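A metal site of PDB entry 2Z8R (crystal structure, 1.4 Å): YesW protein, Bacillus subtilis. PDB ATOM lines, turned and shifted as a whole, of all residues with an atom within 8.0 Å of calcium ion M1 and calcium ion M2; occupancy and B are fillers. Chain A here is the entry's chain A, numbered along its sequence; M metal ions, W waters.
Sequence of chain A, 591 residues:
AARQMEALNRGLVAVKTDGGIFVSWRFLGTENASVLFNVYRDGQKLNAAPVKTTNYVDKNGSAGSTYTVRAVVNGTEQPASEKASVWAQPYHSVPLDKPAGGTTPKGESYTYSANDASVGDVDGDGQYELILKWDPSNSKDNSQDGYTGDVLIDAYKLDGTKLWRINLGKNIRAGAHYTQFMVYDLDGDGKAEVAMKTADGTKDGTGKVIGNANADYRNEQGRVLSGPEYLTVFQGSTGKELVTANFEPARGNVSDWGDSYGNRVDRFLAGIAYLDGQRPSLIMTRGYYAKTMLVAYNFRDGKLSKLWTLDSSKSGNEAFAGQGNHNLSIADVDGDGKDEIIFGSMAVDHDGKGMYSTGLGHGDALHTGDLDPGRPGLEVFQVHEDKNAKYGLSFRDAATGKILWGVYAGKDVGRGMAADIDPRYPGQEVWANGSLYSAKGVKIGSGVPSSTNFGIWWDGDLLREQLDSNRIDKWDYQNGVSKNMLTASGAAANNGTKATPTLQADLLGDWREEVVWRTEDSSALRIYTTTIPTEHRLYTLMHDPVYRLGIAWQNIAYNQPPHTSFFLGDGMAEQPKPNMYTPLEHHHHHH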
ATOM      1  N   ARG A   3     -12.228 -20.331  21.843  1.00  0.00           N
ATOM      2  CA  ARG A   3     -12.334 -20.700  23.258  1.00  0.00           C
ATOM      3  C   ARG A   3     -13.515 -20.040  23.946  1.00  0.00           C
ATOM      4  O   ARG A   3     -13.802 -18.874  23.723  1.00  0.00           O
ATOM      5  CB  ARG A   3     -11.079 -20.279  24.030  1.00  0.00           C
ATOM      6  CG  ARG A   3      -9.901 -21.123  23.795  1.00  0.00           C
ATOM      7  CD  ARG A   3      -8.765 -20.691  24.695  1.00  0.00           C
ATOM      8  NE  ARG A   3      -7.627 -21.551  24.434  1.00  0.00           N
ATOM      9  CZ  ARG A   3      -6.749 -21.945  25.353  1.00  0.00           C
ATOM     10  NH1 ARG A   3      -6.863 -21.550  26.624  1.00  0.00           N
ATOM     11  NH2 ARG A   3      -5.765 -22.751  24.974  1.00  0.00           N
ATOM     12  N   TYR A 274      -7.529 -25.245  29.347  1.00  0.00           N
ATOM     13  CA  TYR A 274      -8.366 -25.681  28.208  1.00  0.00           C
ATOM     14  C   TYR A 274      -7.705 -26.878  27.515  1.00  0.00           C
ATOM     15  O   TYR A 274      -7.078 -26.749  26.448  1.00  0.00           O
ATOM     16  CB  TYR A 274      -8.628 -24.521  27.232  1.00  0.00           C
ATOM     17  CG  TYR A 274      -9.594 -23.500  27.759  1.00  0.00           C
ATOM     18  CD1 TYR A 274     -10.727 -23.134  27.019  1.00  0.00           C
ATOM     19  CD2 TYR A 274      -9.407 -22.888  29.005  1.00  0.00           C
ATOM     20  CE1 TYR A 274     -11.623 -22.177  27.506  1.00  0.00           C
ATOM     21  CE2 TYR A 274     -10.299 -21.944  29.499  1.00  0.00           C
ATOM     22  CZ  TYR A 274     -11.412 -21.597  28.743  1.00  0.00           C
ATOM     23  OH  TYR A 274     -12.299 -20.656  29.215  1.00  0.00           O
ATOM     24  N   LEU A 275      -7.806 -28.041  28.160  1.00  0.00           N
ATOM     25  CA  LEU A 275      -7.140 -29.257  27.679  1.00  0.00           C
ATOM     26  C   LEU A 275      -7.652 -29.731  26.321  1.00  0.00           C
ATOM     27  O   LEU A 275      -6.904 -30.346  25.562  1.00  0.00           O
ATOM     28  CB  LEU A 275      -7.260 -30.381  28.709  1.00  0.00           C
ATOM     29  CG  LEU A 275      -6.727 -30.025  30.101  1.00  0.00           C
ATOM     30  CD1 LEU A 275      -7.108 -31.135  31.076  1.00  0.00           C
ATOM     31  CD2 LEU A 275      -5.207 -29.802  30.104  1.00  0.00           C
ATOM     32  N   GLY A 277      -8.878 -27.526  24.101  1.00  0.00           N
ATOM     33  CA  GLY A 277      -8.719 -26.383  23.189  1.00  0.00           C
ATOM     34  C   GLY A 277      -9.928 -25.480  23.016  1.00  0.00           C
ATOM     35  O   GLY A 277      -9.858 -24.480  22.287  1.00  0.00           O
ATOM     36  N   ALA A 331      -0.620 -22.558  29.628  1.00  0.00           N
ATOM     37  CA  ALA A 331      -0.576 -21.887  28.331  1.00  0.00           C
ATOM     38  C   ALA A 331      -0.512 -22.900  27.210  1.00  0.00           C
ATOM     39  O   ALA A 331      -0.028 -24.000  27.407  1.00  0.00           O
ATOM     40  CB  ALA A 331       0.624 -20.949  28.252  1.00  0.00           C
ATOM     41  N   ASP A 332      -0.981 -22.505  26.044  1.00  0.00           N
ATOM     42  CA  ASP A 332      -0.759 -23.283  24.829  1.00  0.00           C
ATOM     43  C   ASP A 332       0.655 -22.981  24.357  1.00  0.00           C
ATOM     44  O   ASP A 332       0.924 -21.922  23.779  1.00  0.00           O
ATOM     45  CB  ASP A 332      -1.793 -22.923  23.770  1.00  0.00           C
ATOM     46  CG  ASP A 332      -1.546 -23.628  22.454  1.00  0.00           C
ATOM     47  OD1 ASP A 332      -0.726 -24.574  22.397  1.00  0.00           O
ATOM     48  OD2 ASP A 332      -2.185 -23.242  21.462  1.00  0.00           O
ATOM     49  N   VAL A 333       1.574 -23.897  24.662  1.00  0.00           N
ATOM     50  CA  VAL A 333       2.988 -23.678  24.382  1.00  0.00           C
ATOM     51  C   VAL A 333       3.412 -24.295  23.055  1.00  0.00           C
ATOM     52  O   VAL A 333       4.405 -23.879  22.469  1.00  0.00           O
ATOM     53  CB  VAL A 333       3.908 -24.204  25.518  1.00  0.00           C
ATOM     54  CG1 VAL A 333       3.563 -23.545  26.825  1.00  0.00           C
ATOM     55  CG2 VAL A 333       3.827 -25.737  25.635  1.00  0.00           C
ATOM     56  N   ASP A 334       2.661 -25.289  22.580  1.00  0.00           N
ATOM     57  CA  ASP A 334       3.071 -26.028  21.381  1.00  0.00           C
ATOM     58  C   ASP A 334       2.264 -25.685  20.124  1.00  0.00           C
ATOM     59  O   ASP A 334       2.537 -26.188  19.034  1.00  0.00           O
ATOM     60  CB  ASP A 334       3.085 -27.544  21.649  1.00  0.00           C
ATOM     61  CG  ASP A 334       1.731 -28.091  22.087  1.00  0.00           C
ATOM     62  OD1 ASP A 334       0.696 -27.406  21.895  1.00  0.00           O
ATOM     63  OD2 ASP A 334       1.689 -29.228  22.623  1.00  0.00           O
ATOM     64  N   GLY A 335       1.268 -24.802  20.277  1.00  0.00           N
ATOM     65  CA  GLY A 335       0.497 -24.274  19.153  1.00  0.00           C
ATOM     66  C   GLY A 335      -0.664 -25.122  18.642  1.00  0.00           C
ATOM     67  O   GLY A 335      -1.235 -24.800  17.596  1.00  0.00           O
ATOM     68  N   ASP A 336      -1.030 -26.179  19.383  1.00  0.00           N
ATOM     69  CA  ASP A 336      -2.148 -27.054  18.996  1.00  0.00           C
ATOM     70  C   ASP A 336      -3.536 -26.550  19.456  1.00  0.00           C
ATOM     71  O   ASP A 336      -4.552 -27.236  19.255  1.00  0.00           O
ATOM     72  CB  ASP A 336      -1.892 -28.519  19.426  1.00  0.00           C
ATOM     73  CG  ASP A 336      -1.859 -28.706  20.939  1.00  0.00           C
ATOM     74  OD1 ASP A 336      -2.199 -27.756  21.688  1.00  0.00           O
ATOM     75  OD2 ASP A 336      -1.462 -29.817  21.404  1.00  0.00           O
ATOM     76  N   GLY A 337      -3.579 -25.361  20.074  1.00  0.00           N
ATOM     77  CA  GLY A 337      -4.824 -24.765  20.575  1.00  0.00           C
ATOM     78  C   GLY A 337      -5.176 -25.169  22.005  1.00  0.00           C
ATOM     79  O   GLY A 337      -6.019 -24.526  22.665  1.00  0.00           O
ATOM     80  N   LYS A 338      -4.545 -26.239  22.484  1.00  0.00           N
ATOM     81  CA  LYS A 338      -4.848 -26.830  23.783  1.00  0.00           C
ATOM     82  C   LYS A 338      -3.815 -26.351  24.796  1.00  0.00           C
ATOM     83  O   LYS A 338      -2.675 -26.058  24.441  1.00  0.00           O
ATOM     84  CB  LYS A 338      -4.839 -28.353  23.675  1.00  0.00           C
ATOM     85  CG  LYS A 338      -5.718 -28.869  22.546  1.00  0.00           C
ATOM     86  CD  LYS A 338      -5.610 -30.370  22.389  1.00  0.00           C
ATOM     87  CE  LYS A 338      -6.612 -30.863  21.353  1.00  0.00           C
ATOM     88  NZ  LYS A 338      -6.612 -32.358  21.281  1.00  0.00           N
ATOM     89  N   ASP A 339      -4.222 -26.254  26.063  1.00  0.00           N
ATOM     90  CA  ASP A 339      -3.305 -25.800  27.112  1.00  0.00           C
ATOM     91  C   ASP A 339      -2.433 -26.897  27.674  1.00  0.00           C
ATOM     92  O   ASP A 339      -2.885 -28.013  27.952  1.00  0.00           O
ATOM     93  CB  ASP A 339      -4.084 -25.152  28.249  1.00  0.00           C
ATOM     94  CG  ASP A 339      -4.614 -23.796  27.879  1.00  0.00           C
ATOM     95  OD1 ASP A 339      -3.964 -23.071  27.090  1.00  0.00           O
ATOM     96  OD2 ASP A 339      -5.683 -23.439  28.409  1.00  0.00           O
ATOM     97  N   GLU A 340      -1.168 -26.526  27.871  1.00  0.00           N
ATOM     98  CA  GLU A 340      -0.215 -27.338  28.593  1.00  0.00           C
ATOM     99  C   GLU A 340       0.019 -26.710  29.977  1.00  0.00           C
ATOM    100  O   GLU A 340      -0.405 -25.560  30.236  1.00  0.00           O
ATOM    101  CB  GLU A 340       1.096 -27.456  27.807  1.00  0.00           C
ATOM    102  CG  GLU A 340       1.015 -28.355  26.553  1.00  0.00           C
ATOM    103  CD  GLU A 340       0.288 -27.717  25.370  1.00  0.00           C
ATOM    104  OE1 GLU A 340       0.529 -26.543  25.020  1.00  0.00           O
ATOM    105  OE2 GLU A 340      -0.537 -28.431  24.732  1.00  0.00           O
ATOM    106  N   ILE A 341       0.678 -27.457  30.838  1.00  0.00           N
ATOM    107  CA  ILE A 341       0.914 -27.037  32.221  1.00  0.00           C
ATOM    108  C   ILE A 341       2.419 -26.879  32.437  1.00  0.00           C
ATOM    109  O   ILE A 341       3.173 -27.833  32.249  1.00  0.00           O
ATOM    110  CB  ILE A 341       0.346 -28.065  33.215  1.00  0.00           C
ATOM    111  CG1 ILE A 341      -1.165 -28.221  33.006  1.00  0.00           C
ATOM    112  CG2 ILE A 341       0.642 -27.660  34.665  1.00  0.00           C
ATOM    113  CD1 ILE A 341      -1.718 -29.562  33.489  1.00  0.00           C
ATOM    114  N   VAL A 348       3.746 -30.531  31.469  1.00  0.00           N
ATOM    115  CA  VAL A 348       2.799 -31.629  31.276  1.00  0.00           C
ATOM    116  C   VAL A 348       1.897 -31.252  30.117  1.00  0.00           C
ATOM    117  O   VAL A 348       1.394 -30.130  30.070  1.00  0.00           O
ATOM    118  CB  VAL A 348       1.951 -31.886  32.548  1.00  0.00           C
ATOM    119  CG1 VAL A 348       0.963 -33.054  32.322  1.00  0.00           C
ATOM    120  CG2 VAL A 348       2.857 -32.187  33.735  1.00  0.00           C
ATOM    121  N   ASP A 349       1.720 -32.189  29.188  1.00  0.00           N
ATOM    122  CA  ASP A 349       0.917 -31.955  28.001  1.00  0.00           C
ATOM    123  C   ASP A 349      -0.580 -31.962  28.309  1.00  0.00           C
ATOM    124  O   ASP A 349      -0.999 -32.377  29.382  1.00  0.00           O
ATOM    125  CB  ASP A 349       1.225 -33.039  26.955  1.00  0.00           C
ATOM    126  CG  ASP A 349       1.125 -32.537  25.512  1.00  0.00           C
ATOM    127  OD1 ASP A 349       0.613 -31.405  25.267  1.00  0.00           O
ATOM    128  OD2 ASP A 349       1.569 -33.296  24.615  1.00  0.00           O
ATOM    129  N   HIS A 350      -1.368 -31.511  27.334  1.00  0.00           N
ATOM    130  CA  HIS A 350      -2.815 -31.381  27.498  1.00  0.00           C
ATOM    131  C   HIS A 350      -3.510 -32.719  27.784  1.00  0.00           C
ATOM    132  O   HIS A 350      -4.652 -32.747  28.240  1.00  0.00           O
ATOM    133  CB  HIS A 350      -3.418 -30.732  26.251  1.00  0.00           C
ATOM    134  CG  HIS A 350      -3.378 -31.628  25.053  1.00  0.00           C
ATOM    135  ND1 HIS A 350      -2.374 -31.573  24.103  1.00  0.00           N
ATOM    136  CD2 HIS A 350      -4.190 -32.636  24.682  1.00  0.00           C
ATOM    137  CE1 HIS A 350      -2.599 -32.499  23.185  1.00  0.00           C
ATOM    138  NE2 HIS A 350      -3.693 -33.162  23.514  1.00  0.00           N
ATOM    139  N   ASP A 351      -2.821 -33.821  27.479  1.00  0.00           N
ATOM    140  CA  ASP A 351      -3.366 -35.172  27.677  1.00  0.00           C
ATOM    141  C   ASP A 351      -2.785 -35.854  28.919  1.00  0.00           C
ATOM    142  O   ASP A 351      -2.992 -37.035  29.139  1.00  0.00           O
ATOM    143  CB  ASP A 351      -3.089 -36.051  26.451  1.00  0.00           C
ATOM    144  CG  ASP A 351      -1.617 -36.153  26.122  1.00  0.00           C
ATOM    145  OD1 ASP A 351      -0.771 -35.599  26.850  1.00  0.00           O
ATOM    146  OD2 ASP A 351      -1.283 -36.811  25.113  1.00  0.00           O
ATOM    147  N   MET A 355       6.059 -33.862  29.398  1.00  0.00           N
ATOM    148  CA  MET A 355       6.701 -33.340  28.184  1.00  0.00           C
ATOM    149  C   MET A 355       8.212 -33.275  28.279  1.00  0.00           C
ATOM    150  O   MET A 355       8.929 -33.727  27.380  1.00  0.00           O
ATOM    151  CB  MET A 355       6.164 -31.936  27.871  1.00  0.00           C
ATOM    152  CG  MET A 355       4.752 -31.923  27.345  1.00  0.00           C
ATOM    153  SD  MET A 355       3.974 -30.316  27.537  1.00  0.00           S
ATOM    154  CE  MET A 355       5.042 -29.243  26.567  1.00  0.00           C
HETATM  155 CA    CA M   1      -0.945 -26.719  23.165  1.00  0.00          CA
HETATM  156 CA    CA M   2      -0.304 -30.297  23.382  1.00  0.00          CA
HETATM  157  O   HOH W   1       0.570 -32.281  22.339  1.00  0.00           O
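Of the 20 residues printed, 5 come within 4 Å of calcium ion M2. The nearest printed residue that does not touch calcium ion M2 is Lys 338 (4.9 Å).
N of Asp 332 is in hydrogen-bond range of OD1 of Asp 339 (3.2 Å). OD1 of Asp 332 lies close to N of Gly 335 (2.9 Å). The side-chain carboxylate of Asp 332 lies within hydrogen-bond range of the backbone NH of Gly 337 (2.9 Å). N of Asp 349 is in hydrogen-bond range of SD of Met 355. The backbone NH (N) of Glu 340 is in hydrogen-bond range of the backbone carbonyl oxygen (O) of Ala 331 (2.8 Å). The backbone NH (N) of Val 333 sits close to the side-chain carboxylate (OE1) of Glu 340 (2.9 Å).
Calcium ion M2 is bound by the side-chain carboxylate (OE2) of Glu 340 (2.3 Å), the side-chain carboxylate (OD2) of Asp 336 (2.3 Å), the side-chain carboxylate (OD1) of Asp 349 (2.4 Å), the side-chain carboxylate (OD2) of Asp 334 (2.4 Å), water W1 (2.4 Å) and a ring nitrogen (ND1) of His 350 (2.5 Å).
Calcium ion M1 is bound by OD1 of Asp 334 (2.2 Å), OD1 of Asp 336 (2.2 Å), O of Lys 338 (2.2 Å), OD1 of Asp 332 (2.3 Å), OE2 of Glu 340 (2.4 Å) and OE1 of Glu 340 (2.4 Å).
Of the 20 residues printed, 5 come within 4 Å of calcium ion M1. Along chain A the residues within 4 Å of calcium ion M1 span positions 332 to 340.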
